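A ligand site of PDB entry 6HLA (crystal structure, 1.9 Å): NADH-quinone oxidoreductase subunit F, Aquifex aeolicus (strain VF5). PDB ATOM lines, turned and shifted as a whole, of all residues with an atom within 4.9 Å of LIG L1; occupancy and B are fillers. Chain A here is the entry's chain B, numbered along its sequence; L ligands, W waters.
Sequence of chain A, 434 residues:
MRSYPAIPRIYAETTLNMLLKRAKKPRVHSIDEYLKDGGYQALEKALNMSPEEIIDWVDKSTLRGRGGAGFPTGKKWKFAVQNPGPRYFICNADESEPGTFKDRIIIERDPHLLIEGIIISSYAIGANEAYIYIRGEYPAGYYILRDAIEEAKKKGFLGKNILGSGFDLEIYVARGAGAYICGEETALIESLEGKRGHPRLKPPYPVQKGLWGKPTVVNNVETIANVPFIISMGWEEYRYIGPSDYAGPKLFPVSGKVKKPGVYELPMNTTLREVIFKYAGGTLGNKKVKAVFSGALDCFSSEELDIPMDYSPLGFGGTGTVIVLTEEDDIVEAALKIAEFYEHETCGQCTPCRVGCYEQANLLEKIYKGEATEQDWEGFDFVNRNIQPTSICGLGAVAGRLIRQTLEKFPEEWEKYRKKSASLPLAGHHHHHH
O9 of LIG L1 sits at hydrogen-bond distance from O4 of LG2 L2 (2.7 Å).
An oxygen (O6) of LIG L1 is in hydrogen-bond range of the side-chain carboxylate of Glu 185, 2.6 Å away. NZ of Lys 76 is in hydrogen-bond range of O5 of LIG L1. The backbone carbonyl oxygen (O) of Gly 67 lies close to a nitrogen (N7) of LIG L1, 3.2 Å away. An oxygen (O14) of LIG L1 lies within hydrogen-bond range of the backbone NH (N) of Ser 96 (3.2 Å). An oxygen (O14) of LIG L1 lies within hydrogen-bond range of the backbone NH (N) of Glu 97, at 3.2 Å. An oxygen (O12) of LIG L1 sits at hydrogen-bond distance from the backbone carbonyl oxygen of Gly 68 (3.2 Å). The backbone NH (N) of Glu 185 sits at hydrogen-bond distance from an oxygen (O3) of LG2 L2, 3.1 Å away. The side-chain amino group (NZ) of Lys 76 is in salt-bridge range of an oxygen (O8) of LG2 L2 (2.8 Å). An oxygen (O7) of LG2 L2 lies within hydrogen-bond range of the backbone NH (N) of Gly 67, at 2.9 Å. The backbone NH (N) of Glu 95 sits at hydrogen-bond distance from an oxygen (O2) of LG2 L2 (3.0 Å). O9 of LG2 L2 sits at hydrogen-bond distance from N of Asn 220, 2.9 Å away. The side-chain amide nitrogen (ND2) of Asn 220 lies within hydrogen-bond range of an oxygen (O1) of LG2 L2, at 2.8 Å.
Water W2 bridges an oxygen (O13) of LIG L1 (2.7 Å) and the side-chain carboxylate of Glu 97 (2.9 Å). Water W4 bridges O2 of LIG L1 (2.7 Å) and OH of Tyr 205 (2.9 Å). Water W5 lies within hydrogen-bond range of an oxygen (O8) of LIG L1 (2.7 Å), the side-chain carboxylate (OE2) of Glu 184 (2.8 Å) and the backbone NH (N) of Gly 394 (2.9 Å). Water W11 lies within hydrogen-bond range of N7 of LIG L1 and OE2 of Glu 95. Water W8 lies within hydrogen-bond range of OE2 of Glu 185 and O9 of LIG L1. Water W13 lies within hydrogen-bond range of O8 of LG2 L2 (2.7 Å) and N of Phe 71 (2.8 Å).
The side-chain amino group of Lys 76 sits at hydrogen-bond distance from the backbone carbonyl oxygen of Val 218 (2.8 Å). The side-chain carboxylate (OE2) of Glu 97 is in hydrogen-bond range of the side-chain hydroxyl (OH) of Tyr 180 (2.8 Å). The backbone carbonyl oxygen of Glu 97 sits at hydrogen-bond distance from the side-chain hydroxyl of Thr 100 (3.1 Å).
Residues that only touch LIG L1: Ala 69, Phe 71, Phe 79, Glu 95, Tyr 180, Tyr 205, Pro 206, Val 207, Leu 297 and Thr 319. Hydrophobic or aromatic side chains within 4 Å of LIG L1: Ala 69, Phe 71, Phe 79, Tyr 180, Tyr 205, Pro 206, Val 207 and Leu 297. Of the 22 residues printed, 16 come within 4 Å of LIG L1.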
ATOM      1  N   GLY A  67     -33.089 -25.127 -15.603  1.00  0.00           N
ATOM      2  CA  GLY A  67     -31.697 -25.529 -15.715  1.00  0.00           C
ATOM      3  C   GLY A  67     -31.524 -27.011 -15.974  1.00  0.00           C
ATOM      4  O   GLY A  67     -30.454 -27.429 -16.399  1.00  0.00           O
ATOM      5  N   GLY A  68     -32.553 -27.805 -15.692  1.00  0.00           N
ATOM      6  CA  GLY A  68     -32.491 -29.243 -15.917  1.00  0.00           C
ATOM      7  C   GLY A  68     -33.079 -30.116 -14.830  1.00  0.00           C
ATOM      8  O   GLY A  68     -33.576 -31.193 -15.131  1.00  0.00           O
ATOM      9  N   ALA A  69     -33.021 -29.665 -13.558  1.00  0.00           N
ATOM     10  CA  ALA A  69     -33.509 -30.449 -12.416  1.00  0.00           C
ATOM     11  C   ALA A  69     -34.977 -30.223 -12.057  1.00  0.00           C
ATOM     12  O   ALA A  69     -35.545 -31.032 -11.343  1.00  0.00           O
ATOM     13  CB  ALA A  69     -32.626 -30.221 -11.206  1.00  0.00           C
ATOM     14  N   PHE A  71     -36.526 -27.961 -10.045  1.00  0.00           N
ATOM     15  CA  PHE A  71     -36.915 -27.628  -8.668  1.00  0.00           C
ATOM     16  C   PHE A  71     -37.927 -26.472  -8.660  1.00  0.00           C
ATOM     17  O   PHE A  71     -37.725 -25.520  -9.405  1.00  0.00           O
ATOM     18  CB  PHE A  71     -35.702 -27.285  -7.782  1.00  0.00           C
ATOM     19  CG  PHE A  71     -36.033 -27.318  -6.296  1.00  0.00           C
ATOM     20  CD1 PHE A  71     -36.366 -26.149  -5.609  1.00  0.00           C
ATOM     21  CD2 PHE A  71     -36.005 -28.512  -5.590  1.00  0.00           C
ATOM     22  CE1 PHE A  71     -36.710 -26.172  -4.268  1.00  0.00           C
ATOM     23  CE2 PHE A  71     -36.351 -28.540  -4.232  1.00  0.00           C
ATOM     24  CZ  PHE A  71     -36.710 -27.375  -3.579  1.00  0.00           C
ATOM     25  N   LYS A  76     -37.835 -22.652  -3.825  1.00  0.00           N
ATOM     26  CA  LYS A  76     -36.429 -22.314  -3.616  1.00  0.00           C
ATOM     27  C   LYS A  76     -36.279 -20.970  -2.916  1.00  0.00           C
ATOM     28  O   LYS A  76     -35.473 -20.869  -1.996  1.00  0.00           O
ATOM     29  CB  LYS A  76     -35.683 -22.258  -4.947  1.00  0.00           C
ATOM     30  CG  LYS A  76     -34.157 -22.162  -4.737  1.00  0.00           C
ATOM     31  CD  LYS A  76     -33.382 -22.039  -6.032  1.00  0.00           C
ATOM     32  CE  LYS A  76     -33.315 -23.384  -6.677  1.00  0.00           C
ATOM     33  NZ  LYS A  76     -32.613 -23.315  -7.954  1.00  0.00           N
ATOM     34  N   PHE A  79     -37.137 -20.904   0.827  1.00  0.00           N
ATOM     35  CA  PHE A  79     -36.079 -21.398   1.684  1.00  0.00           C
ATOM     36  C   PHE A  79     -35.049 -20.293   1.944  1.00  0.00           C
ATOM     37  O   PHE A  79     -34.622 -20.158   3.089  1.00  0.00           O
ATOM     38  CB  PHE A  79     -35.376 -22.610   1.053  1.00  0.00           C
ATOM     39  CG  PHE A  79     -36.056 -23.950   1.194  1.00  0.00           C
ATOM     40  CD1 PHE A  79     -36.132 -24.577   2.441  1.00  0.00           C
ATOM     41  CD2 PHE A  79     -36.500 -24.641   0.078  1.00  0.00           C
ATOM     42  CE1 PHE A  79     -36.709 -25.848   2.564  1.00  0.00           C
ATOM     43  CE2 PHE A  79     -37.085 -25.911   0.212  1.00  0.00           C
ATOM     44  CZ  PHE A  79     -37.185 -26.507   1.449  1.00  0.00           C
ATOM     45  N   GLU A  95     -24.538 -22.640 -19.261  1.00  0.00           N
ATOM     46  CA  GLU A  95     -25.031 -23.546 -20.328  1.00  0.00           C
ATOM     47  C   GLU A  95     -23.928 -24.302 -21.051  1.00  0.00           C
ATOM     48  O   GLU A  95     -23.345 -23.780 -22.013  1.00  0.00           O
ATOM     49  CB  GLU A  95     -25.905 -22.757 -21.324  1.00  0.00           C
ATOM     50  CG  GLU A  95     -26.516 -23.630 -22.385  1.00  0.00           C
ATOM     51  CD  GLU A  95     -27.581 -22.912 -23.159  1.00  0.00           C
ATOM     52  OE1 GLU A  95     -27.243 -21.929 -23.845  1.00  0.00           O
ATOM     53  OE2 GLU A  95     -28.773 -23.284 -23.025  1.00  0.00           O
ATOM     54  N   SER A  96     -23.562 -25.495 -20.533  1.00  0.00           N
ATOM     55  CA  SER A  96     -22.472 -26.258 -21.139  1.00  0.00           C
ATOM     56  C   SER A  96     -22.816 -27.719 -21.420  1.00  0.00           C
ATOM     57  O   SER A  96     -21.962 -28.479 -21.882  1.00  0.00           O
ATOM     58  CB  SER A  96     -21.219 -26.130 -20.280  1.00  0.00           C
ATOM     59  OG  SER A  96     -20.673 -24.826 -20.402  1.00  0.00           O
ATOM     60  N   GLU A  97     -24.087 -28.108 -21.183  1.00  0.00           N
ATOM     61  CA  GLU A  97     -24.580 -29.440 -21.455  1.00  0.00           C
ATOM     62  C   GLU A  97     -24.578 -29.735 -22.959  1.00  0.00           C
ATOM     63  O   GLU A  97     -25.106 -28.924 -23.710  1.00  0.00           O
ATOM     64  CB  GLU A  97     -26.002 -29.586 -20.894  1.00  0.00           C
ATOM     65  CG  GLU A  97     -26.620 -30.986 -20.986  1.00  0.00           C
ATOM     66  CD  GLU A  97     -26.002 -32.062 -20.116  1.00  0.00           C
ATOM     67  OE1 GLU A  97     -26.556 -33.175 -20.087  1.00  0.00           O
ATOM     68  OE2 GLU A  97     -24.985 -31.788 -19.433  1.00  0.00           O
ATOM     69  N   THR A 100     -27.215 -28.357 -25.720  1.00  0.00           N
ATOM     70  CA  THR A 100     -27.975 -27.312 -25.050  1.00  0.00           C
ATOM     71  C   THR A 100     -27.538 -25.921 -25.470  1.00  0.00           C
ATOM     72  O   THR A 100     -26.448 -25.497 -25.177  1.00  0.00           O
ATOM     73  CB  THR A 100     -27.952 -27.537 -23.545  1.00  0.00           C
ATOM     74  OG1 THR A 100     -28.202 -28.931 -23.292  1.00  0.00           O
ATOM     75  CG2 THR A 100     -28.950 -26.665 -22.799  1.00  0.00           C
ATOM     76  N   TYR A 180     -17.098 -27.167 -17.454  1.00  0.00           N
ATOM     77  CA  TYR A 180     -18.519 -27.550 -17.466  1.00  0.00           C
ATOM     78  C   TYR A 180     -19.078 -27.609 -16.040  1.00  0.00           C
ATOM     79  O   TYR A 180     -20.213 -27.216 -15.805  1.00  0.00           O
ATOM     80  CB  TYR A 180     -18.684 -28.898 -18.175  1.00  0.00           C
ATOM     81  CG  TYR A 180     -19.934 -29.688 -17.876  1.00  0.00           C
ATOM     82  CD1 TYR A 180     -21.140 -29.374 -18.505  1.00  0.00           C
ATOM     83  CD2 TYR A 180     -19.888 -30.801 -17.057  1.00  0.00           C
ATOM     84  CE1 TYR A 180     -22.277 -30.145 -18.286  1.00  0.00           C
ATOM     85  CE2 TYR A 180     -21.019 -31.579 -16.834  1.00  0.00           C
ATOM     86  CZ  TYR A 180     -22.210 -31.254 -17.446  1.00  0.00           C
ATOM     87  OH  TYR A 180     -23.301 -32.066 -17.236  1.00  0.00           O
ATOM     88  N   GLU A 184     -22.473 -26.211 -12.189  1.00  0.00           N
ATOM     89  CA  GLU A 184     -22.946 -26.827 -10.961  1.00  0.00           C
ATOM     90  C   GLU A 184     -22.947 -25.638 -10.014  1.00  0.00           C
ATOM     91  O   GLU A 184     -21.957 -24.894  -9.944  1.00  0.00           O
ATOM     92  CB  GLU A 184     -21.991 -27.953 -10.503  1.00  0.00           C
ATOM     93  CG  GLU A 184     -22.641 -28.914  -9.522  1.00  0.00           C
ATOM     94  CD  GLU A 184     -22.678 -28.465  -8.083  1.00  0.00           C
ATOM     95  OE1 GLU A 184     -21.955 -27.507  -7.726  1.00  0.00           O
ATOM     96  OE2 GLU A 184     -23.429 -29.093  -7.285  1.00  0.00           O
ATOM     97  N   GLU A 185     -24.076 -25.382  -9.390  1.00  0.00           N
ATOM     98  CA  GLU A 185     -24.324 -24.135  -8.640  1.00  0.00           C
ATOM     99  C   GLU A 185     -23.343 -23.845  -7.518  1.00  0.00           C
ATOM    100  O   GLU A 185     -23.126 -22.672  -7.254  1.00  0.00           O
ATOM    101  CB  GLU A 185     -25.748 -24.067  -8.127  1.00  0.00           C
ATOM    102  CG  GLU A 185     -25.995 -25.157  -7.102  1.00  0.00           C
ATOM    103  CD  GLU A 185     -27.349 -25.176  -6.477  1.00  0.00           C
ATOM    104  OE1 GLU A 185     -28.184 -24.287  -6.775  1.00  0.00           O
ATOM    105  OE2 GLU A 185     -27.566 -26.088  -5.636  1.00  0.00           O
ATOM    106  N   TYR A 205     -27.548 -26.166   1.045  1.00  0.00           N
ATOM    107  CA  TYR A 205     -27.912 -25.744  -0.295  1.00  0.00           C
ATOM    108  C   TYR A 205     -27.575 -24.250  -0.350  1.00  0.00           C
ATOM    109  O   TYR A 205     -27.529 -23.629   0.720  1.00  0.00           O
ATOM    110  CB  TYR A 205     -29.386 -26.047  -0.602  1.00  0.00           C
ATOM    111  CG  TYR A 205     -29.617 -27.516  -0.894  1.00  0.00           C
ATOM    112  CD1 TYR A 205     -30.126 -28.371   0.090  1.00  0.00           C
ATOM    113  CD2 TYR A 205     -29.255 -28.074  -2.114  1.00  0.00           C
ATOM    114  CE1 TYR A 205     -30.310 -29.734  -0.158  1.00  0.00           C
ATOM    115  CE2 TYR A 205     -29.432 -29.438  -2.373  1.00  0.00           C
ATOM    116  CZ  TYR A 205     -29.951 -30.257  -1.391  1.00  0.00           C
ATOM    117  OH  TYR A 205     -30.112 -31.606  -1.650  1.00  0.00           O
ATOM    118  N   PRO A 206     -27.306 -23.645  -1.538  1.00  0.00           N
ATOM    119  CA  PRO A 206     -26.923 -22.232  -1.573  1.00  0.00           C
ATOM    120  C   PRO A 206     -27.836 -21.300  -0.813  1.00  0.00           C
ATOM    121  O   PRO A 206     -27.374 -20.294  -0.283  1.00  0.00           O
ATOM    122  CB  PRO A 206     -26.913 -21.911  -3.075  1.00  0.00           C
ATOM    123  CG  PRO A 206     -26.504 -23.186  -3.685  1.00  0.00           C
ATOM    124  CD  PRO A 206     -27.247 -24.228  -2.891  1.00  0.00           C
ATOM    125  N   VAL A 207     -29.135 -21.676  -0.697  1.00  0.00           N
ATOM    126  CA  VAL A 207     -30.187 -20.888  -0.061  1.00  0.00           C
ATOM    127  C   VAL A 207     -29.961 -20.725   1.433  1.00  0.00           C
ATOM    128  O   VAL A 207     -30.469 -19.764   2.020  1.00  0.00           O
ATOM    129  CB  VAL A 207     -31.623 -21.364  -0.402  1.00  0.00           C
ATOM    130  CG1 VAL A 207     -31.982 -21.074  -1.869  1.00  0.00           C
ATOM    131  CG2 VAL A 207     -31.822 -22.838  -0.067  1.00  0.00           C
ATOM    132  N   VAL A 218     -29.696 -19.533  -6.767  1.00  0.00           N
ATOM    133  CA  VAL A 218     -29.108 -19.737  -8.097  1.00  0.00           C
ATOM    134  C   VAL A 218     -30.244 -20.206  -8.980  1.00  0.00           C
ATOM    135  O   VAL A 218     -30.905 -21.188  -8.646  1.00  0.00           O
ATOM    136  CB  VAL A 218     -27.921 -20.741  -8.126  1.00  0.00           C
ATOM    137  CG1 VAL A 218     -27.349 -20.875  -9.534  1.00  0.00           C
ATOM    138  CG2 VAL A 218     -26.828 -20.346  -7.137  1.00  0.00           C
ATOM    139  N   ASN A 220     -31.454 -20.661 -13.294  1.00  0.00           N
ATOM    140  CA  ASN A 220     -31.069 -20.732 -14.692  1.00  0.00           C
ATOM    141  C   ASN A 220     -31.655 -19.519 -15.455  1.00  0.00           C
ATOM    142  O   ASN A 220     -32.666 -18.968 -15.055  1.00  0.00           O
ATOM    143  CB  ASN A 220     -31.620 -22.031 -15.275  1.00  0.00           C
ATOM    144  CG  ASN A 220     -31.467 -22.187 -16.763  1.00  0.00           C
ATOM    145  OD1 ASN A 220     -32.390 -21.945 -17.523  1.00  0.00           O
ATOM    146  ND2 ASN A 220     -30.283 -22.503 -17.219  1.00  0.00           N
ATOM    147  N   LEU A 297     -27.357 -36.724 -20.438  1.00  0.00           N
ATOM    148  CA  LEU A 297     -28.068 -37.272 -19.278  1.00  0.00           C
ATOM    149  C   LEU A 297     -28.856 -38.568 -19.541  1.00  0.00           C
ATOM    150  O   LEU A 297     -28.731 -39.517 -18.772  1.00  0.00           O
ATOM    151  CB  LEU A 297     -28.999 -36.162 -18.725  1.00  0.00           C
ATOM    152  CG  LEU A 297     -29.868 -36.451 -17.490  1.00  0.00           C
ATOM    153  CD1 LEU A 297     -29.022 -36.507 -16.216  1.00  0.00           C
ATOM    154  CD2 LEU A 297     -30.919 -35.372 -17.322  1.00  0.00           C
ATOM    155  N   GLY A 318     -35.225 -33.124 -17.812  1.00  0.00           N
ATOM    156  CA  GLY A 318     -33.922 -32.549 -18.115  1.00  0.00           C
ATOM    157  C   GLY A 318     -34.035 -31.111 -18.563  1.00  0.00           C
ATOM    158  O   GLY A 318     -34.921 -30.394 -18.117  1.00  0.00           O
ATOM    159  N   THR A 319     -33.124 -30.691 -19.472  1.00  0.00           N
ATOM    160  CA  THR A 319     -33.163 -29.315 -19.976  1.00  0.00           C
ATOM    161  C   THR A 319     -34.175 -29.154 -21.122  1.00  0.00           C
ATOM    162  O   THR A 319     -34.411 -28.032 -21.566  1.00  0.00           O
ATOM    163  CB  THR A 319     -31.754 -28.891 -20.456  1.00  0.00           C
ATOM    164  OG1 THR A 319     -31.265 -29.903 -21.329  1.00  0.00           O
ATOM    165  CG2 THR A 319     -30.778 -28.758 -19.329  1.00  0.00           C
ATOM    166  N   GLY A 394     -23.894 -33.724  -9.013  1.00  0.00           N
ATOM    167  CA  GLY A 394     -24.645 -34.486 -10.015  1.00  0.00           C
ATOM    168  C   GLY A 394     -23.832 -35.107 -11.141  1.00  0.00           C
ATOM    169  O   GLY A 394     -24.312 -36.060 -11.748  1.00  0.00           O
HETATM  170  P1  LIG L   1     -30.837 -30.843  -7.844  1.00  0.00           P
HETATM  171  O1  LIG L   1     -32.037 -31.661  -8.151  1.00  0.00           O
HETATM  172  O2  LIG L   1     -30.106 -31.429  -6.657  1.00  0.00           O
HETATM  173  O3  LIG L   1     -31.288 -29.334  -7.395  1.00  0.00           O
HETATM  174  C1  LIG L   1     -31.941 -28.365  -8.235  1.00  0.00           C
HETATM  175  C2  LIG L   1     -31.988 -27.049  -7.506  1.00  0.00           C
HETATM  176  O4  LIG L   1     -32.867 -27.170  -6.371  1.00  0.00           O
HETATM  177  C3  LIG L   1     -30.679 -26.476  -6.970  1.00  0.00           C
HETATM  178  O5  LIG L   1     -30.706 -25.056  -7.057  1.00  0.00           O
HETATM  179  C4  LIG L   1     -30.700 -26.907  -5.497  1.00  0.00           C
HETATM  180  O6  LIG L   1     -29.943 -26.084  -4.615  1.00  0.00           O
HETATM  181  C5  LIG L   1     -32.178 -26.785  -5.184  1.00  0.00           C
HETATM  182  N1  LIG L   1     -32.617 -27.658  -4.102  1.00  0.00           N
HETATM  183  C6  LIG L   1     -32.761 -29.021  -4.164  1.00  0.00           C
HETATM  184  N2  LIG L   1     -33.114 -29.572  -3.027  1.00  0.00           N
HETATM  185  C7  LIG L   1     -33.202 -28.492  -2.158  1.00  0.00           C
HETATM  186  C8  LIG L   1     -33.493 -28.409  -0.784  1.00  0.00           C
HETATM  187  N3  LIG L   1     -33.645 -29.464   0.011  1.00  0.00           N
HETATM  188  N4  LIG L   1     -33.519 -27.176  -0.220  1.00  0.00           N
HETATM  189  C9  LIG L   1     -33.239 -26.112  -0.976  1.00  0.00           C
HETATM  190  N5  LIG L   1     -32.910 -26.075  -2.278  1.00  0.00           N
HETATM  191  C10 LIG L   1     -32.907 -27.305  -2.807  1.00  0.00           C
HETATM  192  O7  LIG L   1     -29.848 -30.878  -9.103  1.00  0.00           O
HETATM  193  P2  LIG L   1     -28.452 -30.254  -9.571  1.00  0.00           P
HETATM  194  O8  LIG L   1     -27.377 -31.200  -9.214  1.00  0.00           O
HETATM  195  O9  LIG L   1     -28.346 -28.859  -9.107  1.00  0.00           O
HETATM  196  O10 LIG L   1     -28.668 -30.252 -11.152  1.00  0.00           O
HETATM  197  C11 LIG L   1     -28.783 -31.451 -11.937  1.00  0.00           C
HETATM  198  C12 LIG L   1     -29.275 -31.039 -13.315  1.00  0.00           C
HETATM  199  O11 LIG L   1     -28.337 -30.138 -13.936  1.00  0.00           O
HETATM  200  C13 LIG L   1     -29.463 -32.177 -14.331  1.00  0.00           C
HETATM  201  O12 LIG L   1     -30.787 -32.678 -14.420  1.00  0.00           O
HETATM  202  C14 LIG L   1     -29.000 -31.569 -15.665  1.00  0.00           C
HETATM  203  O13 LIG L   1     -30.004 -31.521 -16.676  1.00  0.00           O
HETATM  204  C15 LIG L   1     -28.664 -30.122 -15.286  1.00  0.00           C
HETATM  205  N6  LIG L   1     -27.465 -29.565 -16.083  1.00  0.00           N
HETATM  206  C16 LIG L   1     -27.785 -28.536 -16.892  1.00  0.00           C
HETATM  207  C17 LIG L   1     -26.843 -28.014 -17.767  1.00  0.00           C
HETATM  208  C18 LIG L   1     -27.203 -26.890 -18.695  1.00  0.00           C
HETATM  209  O14 LIG L   1     -26.388 -26.539 -19.575  1.00  0.00           O
HETATM  210  N7  LIG L   1     -28.437 -26.373 -18.613  1.00  0.00           N
HETATM  211  C19 LIG L   1     -25.568 -28.562 -17.753  1.00  0.00           C
HETATM  212  C20 LIG L   1     -25.261 -29.630 -16.915  1.00  0.00           C
HETATM  213  C21 LIG L   1     -26.232 -30.114 -16.079  1.00  0.00           C
HETATM  214  N1  LG2 L   2     -27.784 -25.306 -14.374  1.00  0.00           N
HETATM  215  C1  LG2 L   2     -27.784 -24.247 -15.242  1.00  0.00           C
HETATM  216  O1  LG2 L   2     -28.638 -23.363 -15.173  1.00  0.00           O
HETATM  217  N2  LG2 L   2     -26.750 -24.110 -16.169  1.00  0.00           N
HETATM  218  C2  LG2 L   2     -25.644 -24.943 -16.285  1.00  0.00           C
HETATM  219  O2  LG2 L   2     -24.795 -24.718 -17.146  1.00  0.00           O
HETATM  220  C3  LG2 L   2     -25.633 -26.048 -15.321  1.00  0.00           C
HETATM  221  N3  LG2 L   2     -24.579 -26.825 -15.290  1.00  0.00           N
HETATM  222  C4  LG2 L   2     -24.536 -27.835 -14.323  1.00  0.00           C
HETATM  223  C5  LG2 L   2     -23.442 -28.710 -14.308  1.00  0.00           C
HETATM  224  C6  LG2 L   2     -23.402 -29.791 -13.437  1.00  0.00           C
HETATM  225  C7  LG2 L   2     -22.221 -30.731 -13.476  1.00  0.00           C
HETATM  226  C8  LG2 L   2     -24.464 -29.990 -12.538  1.00  0.00           C
HETATM  227  C9  LG2 L   2     -24.476 -31.167 -11.581  1.00  0.00           C
HETATM  228  C10 LG2 L   2     -25.536 -29.104 -12.524  1.00  0.00           C
HETATM  229  C11 LG2 L   2     -25.583 -28.029 -13.415  1.00  0.00           C
HETATM  230  N4  LG2 L   2     -26.702 -27.140 -13.465  1.00  0.00           N
HETATM  231  C12 LG2 L   2     -26.762 -26.145 -14.408  1.00  0.00           C
HETATM  232  C13 LG2 L   2     -27.746 -27.197 -12.435  1.00  0.00           C
HETATM  233  C14 LG2 L   2     -27.486 -26.232 -11.279  1.00  0.00           C
HETATM  234  O3  LG2 L   2     -26.603 -26.843 -10.329  1.00  0.00           O
HETATM  235  C15 LG2 L   2     -28.793 -25.785 -10.629  1.00  0.00           C
HETATM  236  O4  LG2 L   2     -29.676 -26.903 -10.473  1.00  0.00           O
HETATM  237  C16 LG2 L   2     -29.565 -24.682 -11.365  1.00  0.00           C
HETATM  238  O5  LG2 L   2     -28.704 -23.671 -11.903  1.00  0.00           O
HETATM  239  C17 LG2 L   2     -30.622 -24.068 -10.487  1.00  0.00           C
HETATM  240  O6  LG2 L   2     -31.480 -23.253 -11.315  1.00  0.00           O
HETATM  241  P1  LG2 L   2     -32.933 -23.660 -11.733  1.00  0.00           P
HETATM  242  O7  LG2 L   2     -32.906 -24.725 -12.736  1.00  0.00           O
HETATM  243  O8  LG2 L   2     -33.629 -24.148 -10.443  1.00  0.00           O
HETATM  244  O9  LG2 L   2     -33.608 -22.359 -12.233  1.00  0.00           O
HETATM  245  O   HOH W   1     -27.803 -31.028  -5.466  1.00  0.00           O
HETATM  246  O   HOH W   2     -29.136 -32.701 -18.899  1.00  0.00           O
HETATM  247  O   HOH W   3     -32.221 -33.826  -9.935  1.00  0.00           O
HETATM  248  O   HOH W   4     -30.653 -32.587  -4.283  1.00  0.00           O
HETATM  249  O   HOH W   5     -24.986 -31.273  -7.934  1.00  0.00           O
HETATM  250  O   HOH W   6     -25.510 -33.302 -15.432  1.00  0.00           O
HETATM  251  O   HOH W   7     -31.066 -24.150  -3.174  1.00  0.00           O
HETATM  252  O   HOH W   8     -27.092 -28.628  -6.538  1.00  0.00           O
HETATM  253  O   HOH W   9     -33.404 -27.058   2.600  1.00  0.00           O
HETATM  254  O   HOH W  10     -30.945 -34.389 -12.296  1.00  0.00           O
HETATM  255  O   HOH W  11     -29.345 -24.313 -20.285  1.00  0.00           O
HETATM  256  O   HOH W  12     -33.557 -32.430  -2.933  1.00  0.00           O
HETATM  257  O   HOH W  13     -34.003 -26.844 -10.498  1.00  0.00           O
HETATM  258  O   HOH W  14     -28.059 -33.832  -9.094  1.00  0.00           O
